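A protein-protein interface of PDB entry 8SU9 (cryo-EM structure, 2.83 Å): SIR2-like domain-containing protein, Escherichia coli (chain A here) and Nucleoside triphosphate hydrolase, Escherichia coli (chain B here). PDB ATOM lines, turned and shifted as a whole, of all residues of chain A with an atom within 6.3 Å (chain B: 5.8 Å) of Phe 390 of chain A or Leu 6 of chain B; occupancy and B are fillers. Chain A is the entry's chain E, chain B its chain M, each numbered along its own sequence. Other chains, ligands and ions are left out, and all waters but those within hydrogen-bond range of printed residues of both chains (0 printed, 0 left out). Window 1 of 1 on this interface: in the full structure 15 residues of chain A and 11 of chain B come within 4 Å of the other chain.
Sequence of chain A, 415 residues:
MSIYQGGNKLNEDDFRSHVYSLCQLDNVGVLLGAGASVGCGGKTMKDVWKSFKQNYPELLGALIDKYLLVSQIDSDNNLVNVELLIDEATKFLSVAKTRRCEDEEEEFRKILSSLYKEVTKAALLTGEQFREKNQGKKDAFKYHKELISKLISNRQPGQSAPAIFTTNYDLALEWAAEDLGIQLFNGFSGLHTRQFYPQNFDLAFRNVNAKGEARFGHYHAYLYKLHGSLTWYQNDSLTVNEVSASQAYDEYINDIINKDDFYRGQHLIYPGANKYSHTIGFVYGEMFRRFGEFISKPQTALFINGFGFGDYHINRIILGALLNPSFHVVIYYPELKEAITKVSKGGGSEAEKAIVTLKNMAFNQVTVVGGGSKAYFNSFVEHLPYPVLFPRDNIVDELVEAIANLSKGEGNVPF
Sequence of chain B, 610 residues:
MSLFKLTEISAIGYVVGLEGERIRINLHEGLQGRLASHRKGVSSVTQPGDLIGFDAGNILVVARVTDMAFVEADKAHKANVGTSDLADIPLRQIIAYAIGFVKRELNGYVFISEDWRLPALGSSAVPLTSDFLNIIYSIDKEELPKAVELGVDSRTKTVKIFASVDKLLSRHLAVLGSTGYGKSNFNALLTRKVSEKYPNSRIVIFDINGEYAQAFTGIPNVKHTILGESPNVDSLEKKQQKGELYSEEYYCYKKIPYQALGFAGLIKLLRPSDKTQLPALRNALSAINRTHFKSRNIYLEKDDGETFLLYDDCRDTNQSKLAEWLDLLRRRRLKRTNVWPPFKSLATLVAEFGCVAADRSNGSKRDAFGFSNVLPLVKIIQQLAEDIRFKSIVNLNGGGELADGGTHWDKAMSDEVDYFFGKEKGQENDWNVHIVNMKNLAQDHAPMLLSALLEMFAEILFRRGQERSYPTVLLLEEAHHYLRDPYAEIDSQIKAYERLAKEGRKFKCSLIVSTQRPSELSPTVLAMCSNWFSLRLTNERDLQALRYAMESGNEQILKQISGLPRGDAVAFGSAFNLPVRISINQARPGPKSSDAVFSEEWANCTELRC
The backbone carbonyl oxygen of Pro 387 of chain A sits at hydrogen-bond distance from the guanidinium group of Arg 104 of chain B, at 3.4 Å. The backbone carbonyl oxygen (O) of Leu 6 of chain B lies close to the backbone carbonyl oxygen (O) of Leu 389 of chain A. The guanidinium group of Arg 392 of chain A lies close to the guanidinium group of Arg 104 of chain B.
The side-chain hydroxyl (OG) of Ser 153 of chain A lies close to the backbone carbonyl oxygen (O) of Ser 149 of chain A (3.4 Å).
OG of Ser 149 of chain A touches CE1 of Phe 4 of chain B, 3.9 Å away. Ser 153 of chain A touches Phe 4 of chain B. Tyr 219 of chain A touches Leu 6 of chain B (OH to CB, 3.3 Å). Arg 104 of chain B touches Tyr 386 of chain A (NE to CD2, 3.3 Å). Val 388 of chain A touches Arg 104 of chain B. CD1 of Leu 389 of chain A touches CG2 of Thr 7 of chain B, at 3.99 Å. Leu 389 of chain A touches Asp 55 of chain B. CA of Phe 390 of chain A touches O of Leu 6 of chain B, 3.99 Å away. Lys 5 of chain B touches Pro 391 of chain A (O to CD, 3.6 Å). Leu 6 of chain B touches Pro 391 of chain A.
Printed residues of chain B within 4 Å of Phe 390 of chain A: Leu 6 (3.99 Å). Printed residues of chain A within 4 Å of Leu 6 of chain B: Ser 153 (3.5 Å), Tyr 219 (3.3 Å), Leu 389 (3.5 Å), Phe 390 (3.99 Å) and Pro 391 (3.97 Å). Of the printed residues of chain B, Ser 153 of chain A touches Phe 4 and Leu 6. Printed residues of chain B within 4 Å of Tyr 219 of chain A: Leu 6. Of the printed residues of chain B, Tyr 386 of chain A touches Arg 104 (3.3 Å). Printed residues of chain B within 4 Å of Pro 387 of chain A: Arg 104. Of the printed residues of chain B, Pro 391 of chain A touches Lys 5 and Leu 6. Asn 154 of chain A touches none of the printed residues of chain B. The nearest printed residue of chain A that does not touch Leu 6 of chain B is Ile 152 of chain A (4.9 Å).
Of the 7 printed residues of chain B, 6 touch a printed residue of chain A. Hydrophobic or aromatic side chains of chain B that line the printed part of chain A: Phe 4 and Leu 6. Printed residues of chain A that touch a printed residue of chain B: Ser 149, Ser 153, Tyr 219, Tyr 386, Pro 387, Val 388, Leu 389, Phe 390, Pro 391 and Arg 392. Hydrophobic or aromatic side chains of chain A that line the printed part of chain B: Tyr 219, Tyr 386, Leu 389 and Pro 391. Among the printed residues, no Asp or Glu carboxylate lies within 4 Å of a Lys or Arg side-chain nitrogen of the other chain.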
ATOM      1  N   SER A 149     -24.080 -26.107 -20.879  1.00  0.00           N
ATOM      2  CA  SER A 149     -24.720 -25.343 -21.945  1.00  0.00           C
ATOM      3  C   SER A 149     -26.207 -25.652 -22.040  1.00  0.00           C
ATOM      4  O   SER A 149     -27.023 -24.746 -22.244  1.00  0.00           O
ATOM      5  CB  SER A 149     -24.028 -25.623 -23.276  1.00  0.00           C
ATOM      6  OG  SER A 149     -24.781 -25.100 -24.352  1.00  0.00           O
ATOM      7  N   ILE A 152     -28.287 -23.931 -19.084  1.00  0.00           N
ATOM      8  CA  ILE A 152     -28.470 -22.484 -19.163  1.00  0.00           C
ATOM      9  C   ILE A 152     -29.403 -22.108 -20.309  1.00  0.00           C
ATOM     10  O   ILE A 152     -30.283 -21.253 -20.155  1.00  0.00           O
ATOM     11  CB  ILE A 152     -27.104 -21.788 -19.296  1.00  0.00           C
ATOM     12  CG1 ILE A 152     -26.409 -21.719 -17.939  1.00  0.00           C
ATOM     13  CG2 ILE A 152     -27.257 -20.396 -19.885  1.00  0.00           C
ATOM     14  CD1 ILE A 152     -25.001 -21.198 -18.011  1.00  0.00           C
ATOM     15  N   SER A 153     -29.240 -22.742 -21.467  1.00  0.00           N
ATOM     16  CA  SER A 153     -29.828 -22.259 -22.712  1.00  0.00           C
ATOM     17  C   SER A 153     -31.294 -22.635 -22.893  1.00  0.00           C
ATOM     18  O   SER A 153     -31.790 -22.564 -24.021  1.00  0.00           O
ATOM     19  CB  SER A 153     -29.020 -22.776 -23.904  1.00  0.00           C
ATOM     20  OG  SER A 153     -27.864 -21.985 -24.114  1.00  0.00           O
ATOM     21  N   ASN A 154     -32.006 -23.025 -21.840  1.00  0.00           N
ATOM     22  CA  ASN A 154     -33.432 -23.310 -21.962  1.00  0.00           C
ATOM     23  C   ASN A 154     -34.205 -22.699 -20.802  1.00  0.00           C
ATOM     24  O   ASN A 154     -35.126 -23.313 -20.255  1.00  0.00           O
ATOM     25  CB  ASN A 154     -33.698 -24.812 -22.068  1.00  0.00           C
ATOM     26  CG  ASN A 154     -33.005 -25.612 -20.988  1.00  0.00           C
ATOM     27  OD1 ASN A 154     -32.876 -25.168 -19.848  1.00  0.00           O
ATOM     28  ND2 ASN A 154     -32.555 -26.809 -21.345  1.00  0.00           N
ATOM     29  N   TYR A 219     -25.997 -15.041 -17.790  1.00  0.00           N
ATOM     30  CA  TYR A 219     -25.116 -16.201 -17.928  1.00  0.00           C
ATOM     31  C   TYR A 219     -24.371 -16.397 -16.613  1.00  0.00           C
ATOM     32  O   TYR A 219     -23.247 -15.916 -16.448  1.00  0.00           O
ATOM     33  CB  TYR A 219     -24.153 -16.017 -19.098  1.00  0.00           C
ATOM     34  CG  TYR A 219     -24.834 -15.876 -20.441  1.00  0.00           C
ATOM     35  CD1 TYR A 219     -25.986 -16.591 -20.736  1.00  0.00           C
ATOM     36  CD2 TYR A 219     -24.324 -15.026 -21.413  1.00  0.00           C
ATOM     37  CE1 TYR A 219     -26.612 -16.466 -21.962  1.00  0.00           C
ATOM     38  CE2 TYR A 219     -24.942 -14.893 -22.642  1.00  0.00           C
ATOM     39  CZ  TYR A 219     -26.085 -15.615 -22.910  1.00  0.00           C
ATOM     40  OH  TYR A 219     -26.704 -15.485 -24.132  1.00  0.00           O
ATOM     41  N   TYR A 386     -32.427 -30.215 -26.678  1.00  0.00           N
ATOM     42  CA  TYR A 386     -31.422 -29.411 -27.357  1.00  0.00           C
ATOM     43  C   TYR A 386     -32.078 -28.165 -27.936  1.00  0.00           C
ATOM     44  O   TYR A 386     -33.093 -28.283 -28.639  1.00  0.00           O
ATOM     45  CB  TYR A 386     -30.754 -30.227 -28.461  1.00  0.00           C
ATOM     46  CG  TYR A 386     -29.448 -29.656 -28.960  1.00  0.00           C
ATOM     47  CD1 TYR A 386     -28.245 -29.992 -28.352  1.00  0.00           C
ATOM     48  CD2 TYR A 386     -29.414 -28.792 -30.046  1.00  0.00           C
ATOM     49  CE1 TYR A 386     -27.047 -29.478 -28.807  1.00  0.00           C
ATOM     50  CE2 TYR A 386     -28.220 -28.272 -30.509  1.00  0.00           C
ATOM     51  CZ  TYR A 386     -27.039 -28.619 -29.885  1.00  0.00           C
ATOM     52  OH  TYR A 386     -25.847 -28.106 -30.341  1.00  0.00           O
ATOM     53  N   PRO A 387     -31.555 -26.971 -27.675  1.00  0.00           N
ATOM     54  CA  PRO A 387     -32.223 -25.752 -28.146  1.00  0.00           C
ATOM     55  C   PRO A 387     -32.155 -25.604 -29.658  1.00  0.00           C
ATOM     56  O   PRO A 387     -31.241 -26.104 -30.318  1.00  0.00           O
ATOM     57  CB  PRO A 387     -31.453 -24.626 -27.443  1.00  0.00           C
ATOM     58  CG  PRO A 387     -30.586 -25.301 -26.417  1.00  0.00           C
ATOM     59  CD  PRO A 387     -30.327 -26.671 -26.926  1.00  0.00           C
ATOM     60  N   VAL A 388     -33.148 -24.900 -30.204  1.00  0.00           N
ATOM     61  CA  VAL A 388     -33.240 -24.731 -31.653  1.00  0.00           C
ATOM     62  C   VAL A 388     -32.202 -23.736 -32.157  1.00  0.00           C
ATOM     63  O   VAL A 388     -31.531 -23.979 -33.166  1.00  0.00           O
ATOM     64  CB  VAL A 388     -34.664 -24.308 -32.052  1.00  0.00           C
ATOM     65  CG1 VAL A 388     -34.799 -24.279 -33.560  1.00  0.00           C
ATOM     66  CG2 VAL A 388     -35.679 -25.254 -31.456  1.00  0.00           C
ATOM     67  N   LEU A 389     -32.051 -22.607 -31.470  1.00  0.00           N
ATOM     68  CA  LEU A 389     -31.198 -21.530 -31.959  1.00  0.00           C
ATOM     69  C   LEU A 389     -29.726 -21.723 -31.622  1.00  0.00           C
ATOM     70  O   LEU A 389     -28.909 -20.880 -32.006  1.00  0.00           O
ATOM     71  CB  LEU A 389     -31.678 -20.186 -31.407  1.00  0.00           C
ATOM     72  CG  LEU A 389     -32.810 -19.515 -32.187  1.00  0.00           C
ATOM     73  CD1 LEU A 389     -33.363 -18.326 -31.421  1.00  0.00           C
ATOM     74  CD2 LEU A 389     -32.328 -19.090 -33.561  1.00  0.00           C
ATOM     75  N   PHE A 390     -29.370 -22.789 -30.919  1.00  0.00           N
ATOM     76  CA  PHE A 390     -27.969 -23.042 -30.620  1.00  0.00           C
ATOM     77  C   PHE A 390     -27.212 -23.312 -31.918  1.00  0.00           C
ATOM     78  O   PHE A 390     -27.649 -24.144 -32.723  1.00  0.00           O
ATOM     79  CB  PHE A 390     -27.834 -24.231 -29.668  1.00  0.00           C
ATOM     80  CG  PHE A 390     -26.455 -24.403 -29.096  1.00  0.00           C
ATOM     81  CD1 PHE A 390     -25.470 -25.067 -29.807  1.00  0.00           C
ATOM     82  CD2 PHE A 390     -26.148 -23.909 -27.841  1.00  0.00           C
ATOM     83  CE1 PHE A 390     -24.202 -25.228 -29.281  1.00  0.00           C
ATOM     84  CE2 PHE A 390     -24.884 -24.067 -27.308  1.00  0.00           C
ATOM     85  CZ  PHE A 390     -23.910 -24.726 -28.029  1.00  0.00           C
ATOM     86  N   PRO A 391     -26.089 -22.638 -32.159  1.00  0.00           N
ATOM     87  CA  PRO A 391     -25.360 -22.815 -33.423  1.00  0.00           C
ATOM     88  C   PRO A 391     -24.618 -24.143 -33.455  1.00  0.00           C
ATOM     89  O   PRO A 391     -23.609 -24.329 -32.768  1.00  0.00           O
ATOM     90  CB  PRO A 391     -24.397 -21.619 -33.435  1.00  0.00           C
ATOM     91  CG  PRO A 391     -24.171 -21.309 -31.995  1.00  0.00           C
ATOM     92  CD  PRO A 391     -25.435 -21.667 -31.264  1.00  0.00           C
ATOM     93  N   ARG A 392     -25.123 -25.077 -34.259  1.00  0.00           N
ATOM     94  CA  ARG A 392     -24.488 -26.383 -34.423  1.00  0.00           C
ATOM     95  C   ARG A 392     -23.658 -26.391 -35.706  1.00  0.00           C
ATOM     96  O   ARG A 392     -23.940 -27.099 -36.674  1.00  0.00           O
ATOM     97  CB  ARG A 392     -25.540 -27.489 -34.420  1.00  0.00           C
ATOM     98  CG  ARG A 392     -24.969 -28.885 -34.213  1.00  0.00           C
ATOM     99  CD  ARG A 392     -26.033 -29.956 -34.391  1.00  0.00           C
ATOM    100  NE  ARG A 392     -26.765 -30.212 -33.156  1.00  0.00           N
ATOM    101  CZ  ARG A 392     -27.501 -31.291 -32.932  1.00  0.00           C
ATOM    102  NH1 ARG A 392     -27.627 -32.244 -33.842  1.00  0.00           N
ATOM    103  NH2 ARG A 392     -28.128 -31.418 -31.766  1.00  0.00           N
ATOM    104  N   ASP A 393     -22.608 -25.575 -35.691  1.00  0.00           N
ATOM    105  CA  ASP A 393     -21.699 -25.450 -36.825  1.00  0.00           C
ATOM    106  C   ASP A 393     -20.360 -24.939 -36.309  1.00  0.00           C
ATOM    107  O   ASP A 393     -20.157 -24.776 -35.102  1.00  0.00           O
ATOM    108  CB  ASP A 393     -22.278 -24.529 -37.903  1.00  0.00           C
ATOM    109  CG  ASP A 393     -23.111 -25.276 -38.925  1.00  0.00           C
ATOM    110  OD1 ASP A 393     -22.682 -26.364 -39.364  1.00  0.00           O
ATOM    111  OD2 ASP A 393     -24.195 -24.775 -39.291  1.00  0.00           O
ATOM    112  N   PHE B   4     -19.196 -17.599 -24.906  1.00  0.00           N
ATOM    113  CA  PHE B   4     -20.471 -18.281 -25.070  1.00  0.00           C
ATOM    114  C   PHE B   4     -21.350 -17.501 -26.039  1.00  0.00           C
ATOM    115  O   PHE B   4     -21.543 -16.292 -25.879  1.00  0.00           O
ATOM    116  CB  PHE B   4     -21.178 -18.437 -23.722  1.00  0.00           C
ATOM    117  CG  PHE B   4     -22.354 -19.371 -23.758  1.00  0.00           C
ATOM    118  CD1 PHE B   4     -22.195 -20.692 -24.147  1.00  0.00           C
ATOM    119  CD2 PHE B   4     -23.618 -18.931 -23.401  1.00  0.00           C
ATOM    120  CE1 PHE B   4     -23.274 -21.554 -24.181  1.00  0.00           C
ATOM    121  CE2 PHE B   4     -24.700 -19.790 -23.433  1.00  0.00           C
ATOM    122  CZ  PHE B   4     -24.528 -21.103 -23.824  1.00  0.00           C
ATOM    123  N   LYS B   5     -21.880 -18.198 -27.041  1.00  0.00           N
ATOM    124  CA  LYS B   5     -22.745 -17.601 -28.058  1.00  0.00           C
ATOM    125  C   LYS B   5     -24.050 -18.388 -28.082  1.00  0.00           C
ATOM    126  O   LYS B   5     -24.123 -19.467 -28.677  1.00  0.00           O
ATOM    127  CB  LYS B   5     -22.065 -17.600 -29.423  1.00  0.00           C
ATOM    128  CG  LYS B   5     -22.700 -16.658 -30.431  1.00  0.00           C
ATOM    129  CD  LYS B   5     -22.555 -15.208 -30.000  1.00  0.00           C
ATOM    130  CE  LYS B   5     -22.766 -14.262 -31.171  1.00  0.00           C
ATOM    131  NZ  LYS B   5     -23.224 -12.918 -30.723  1.00  0.00           N
ATOM    132  N   LEU B   6     -25.083 -17.845 -27.435  1.00  0.00           N
ATOM    133  CA  LEU B   6     -26.368 -18.530 -27.380  1.00  0.00           C
ATOM    134  C   LEU B   6     -27.131 -18.416 -28.695  1.00  0.00           C
ATOM    135  O   LEU B   6     -27.821 -19.362 -29.089  1.00  0.00           O
ATOM    136  CB  LEU B   6     -27.203 -17.980 -26.219  1.00  0.00           C
ATOM    137  CG  LEU B   6     -28.435 -18.758 -25.747  1.00  0.00           C
ATOM    138  CD1 LEU B   6     -28.642 -18.543 -24.256  1.00  0.00           C
ATOM    139  CD2 LEU B   6     -29.686 -18.355 -26.508  1.00  0.00           C
ATOM    140  N   THR B   7     -27.021 -17.278 -29.381  1.00  0.00           N
ATOM    141  CA  THR B   7     -27.676 -17.073 -30.666  1.00  0.00           C
ATOM    142  C   THR B   7     -26.697 -16.444 -31.645  1.00  0.00           C
ATOM    143  O   THR B   7     -25.864 -15.618 -31.259  1.00  0.00           O
ATOM    144  CB  THR B   7     -28.918 -16.177 -30.541  1.00  0.00           C
ATOM    145  OG1 THR B   7     -28.570 -14.960 -29.866  1.00  0.00           O
ATOM    146  CG2 THR B   7     -30.026 -16.885 -29.777  1.00  0.00           C
ATOM    147  N   GLU B   8     -26.806 -16.839 -32.914  1.00  0.00           N
ATOM    148  CA  GLU B   8     -26.008 -16.270 -33.993  1.00  0.00           C
ATOM    149  C   GLU B   8     -26.816 -15.295 -34.846  1.00  0.00           C
ATOM    150  O   GLU B   8     -26.518 -15.105 -36.030  1.00  0.00           O
ATOM    151  CB  GLU B   8     -25.424 -17.383 -34.863  1.00  0.00           C
ATOM    152  CG  GLU B   8     -24.097 -17.038 -35.529  1.00  0.00           C
ATOM    153  CD  GLU B   8     -22.928 -17.070 -34.562  1.00  0.00           C
ATOM    154  OE1 GLU B   8     -23.076 -17.654 -33.467  1.00  0.00           O
ATOM    155  OE2 GLU B   8     -21.863 -16.511 -34.896  1.00  0.00           O
ATOM    156  N   ASP B  55     -37.855 -16.265 -29.583  1.00  0.00           N
ATOM    157  CA  ASP B  55     -37.096 -17.324 -28.924  1.00  0.00           C
ATOM    158  C   ASP B  55     -37.713 -17.599 -27.557  1.00  0.00           C
ATOM    159  O   ASP B  55     -37.592 -16.787 -26.635  1.00  0.00           O
ATOM    160  CB  ASP B  55     -35.623 -16.940 -28.804  1.00  0.00           C
ATOM    161  CG  ASP B  55     -35.424 -15.542 -28.253  1.00  0.00           C
ATOM    162  OD1 ASP B  55     -36.402 -14.767 -28.226  1.00  0.00           O
ATOM    163  OD2 ASP B  55     -34.288 -15.219 -27.847  1.00  0.00           O
ATOM    164  N   ARG B 104     -37.272 -29.203 -32.763  1.00  0.00           N
ATOM    165  CA  ARG B 104     -36.148 -30.066 -33.104  1.00  0.00           C
ATOM    166  C   ARG B 104     -36.314 -31.389 -32.374  1.00  0.00           C
ATOM    167  O   ARG B 104     -36.486 -31.403 -31.150  1.00  0.00           O
ATOM    168  CB  ARG B 104     -34.823 -29.407 -32.717  1.00  0.00           C
ATOM    169  CG  ARG B 104     -33.592 -30.171 -33.138  1.00  0.00           C
ATOM    170  CD  ARG B 104     -32.461 -29.938 -32.157  1.00  0.00           C
ATOM    171  NE  ARG B 104     -31.710 -28.726 -32.456  1.00  0.00           N
ATOM    172  CZ  ARG B 104     -30.645 -28.682 -33.241  1.00  0.00           C
ATOM    173  NH1 ARG B 104     -30.177 -29.767 -33.834  1.00  0.00           N
ATOM    174  NH2 ARG B 104     -30.030 -27.518 -33.437  1.00  0.00           N
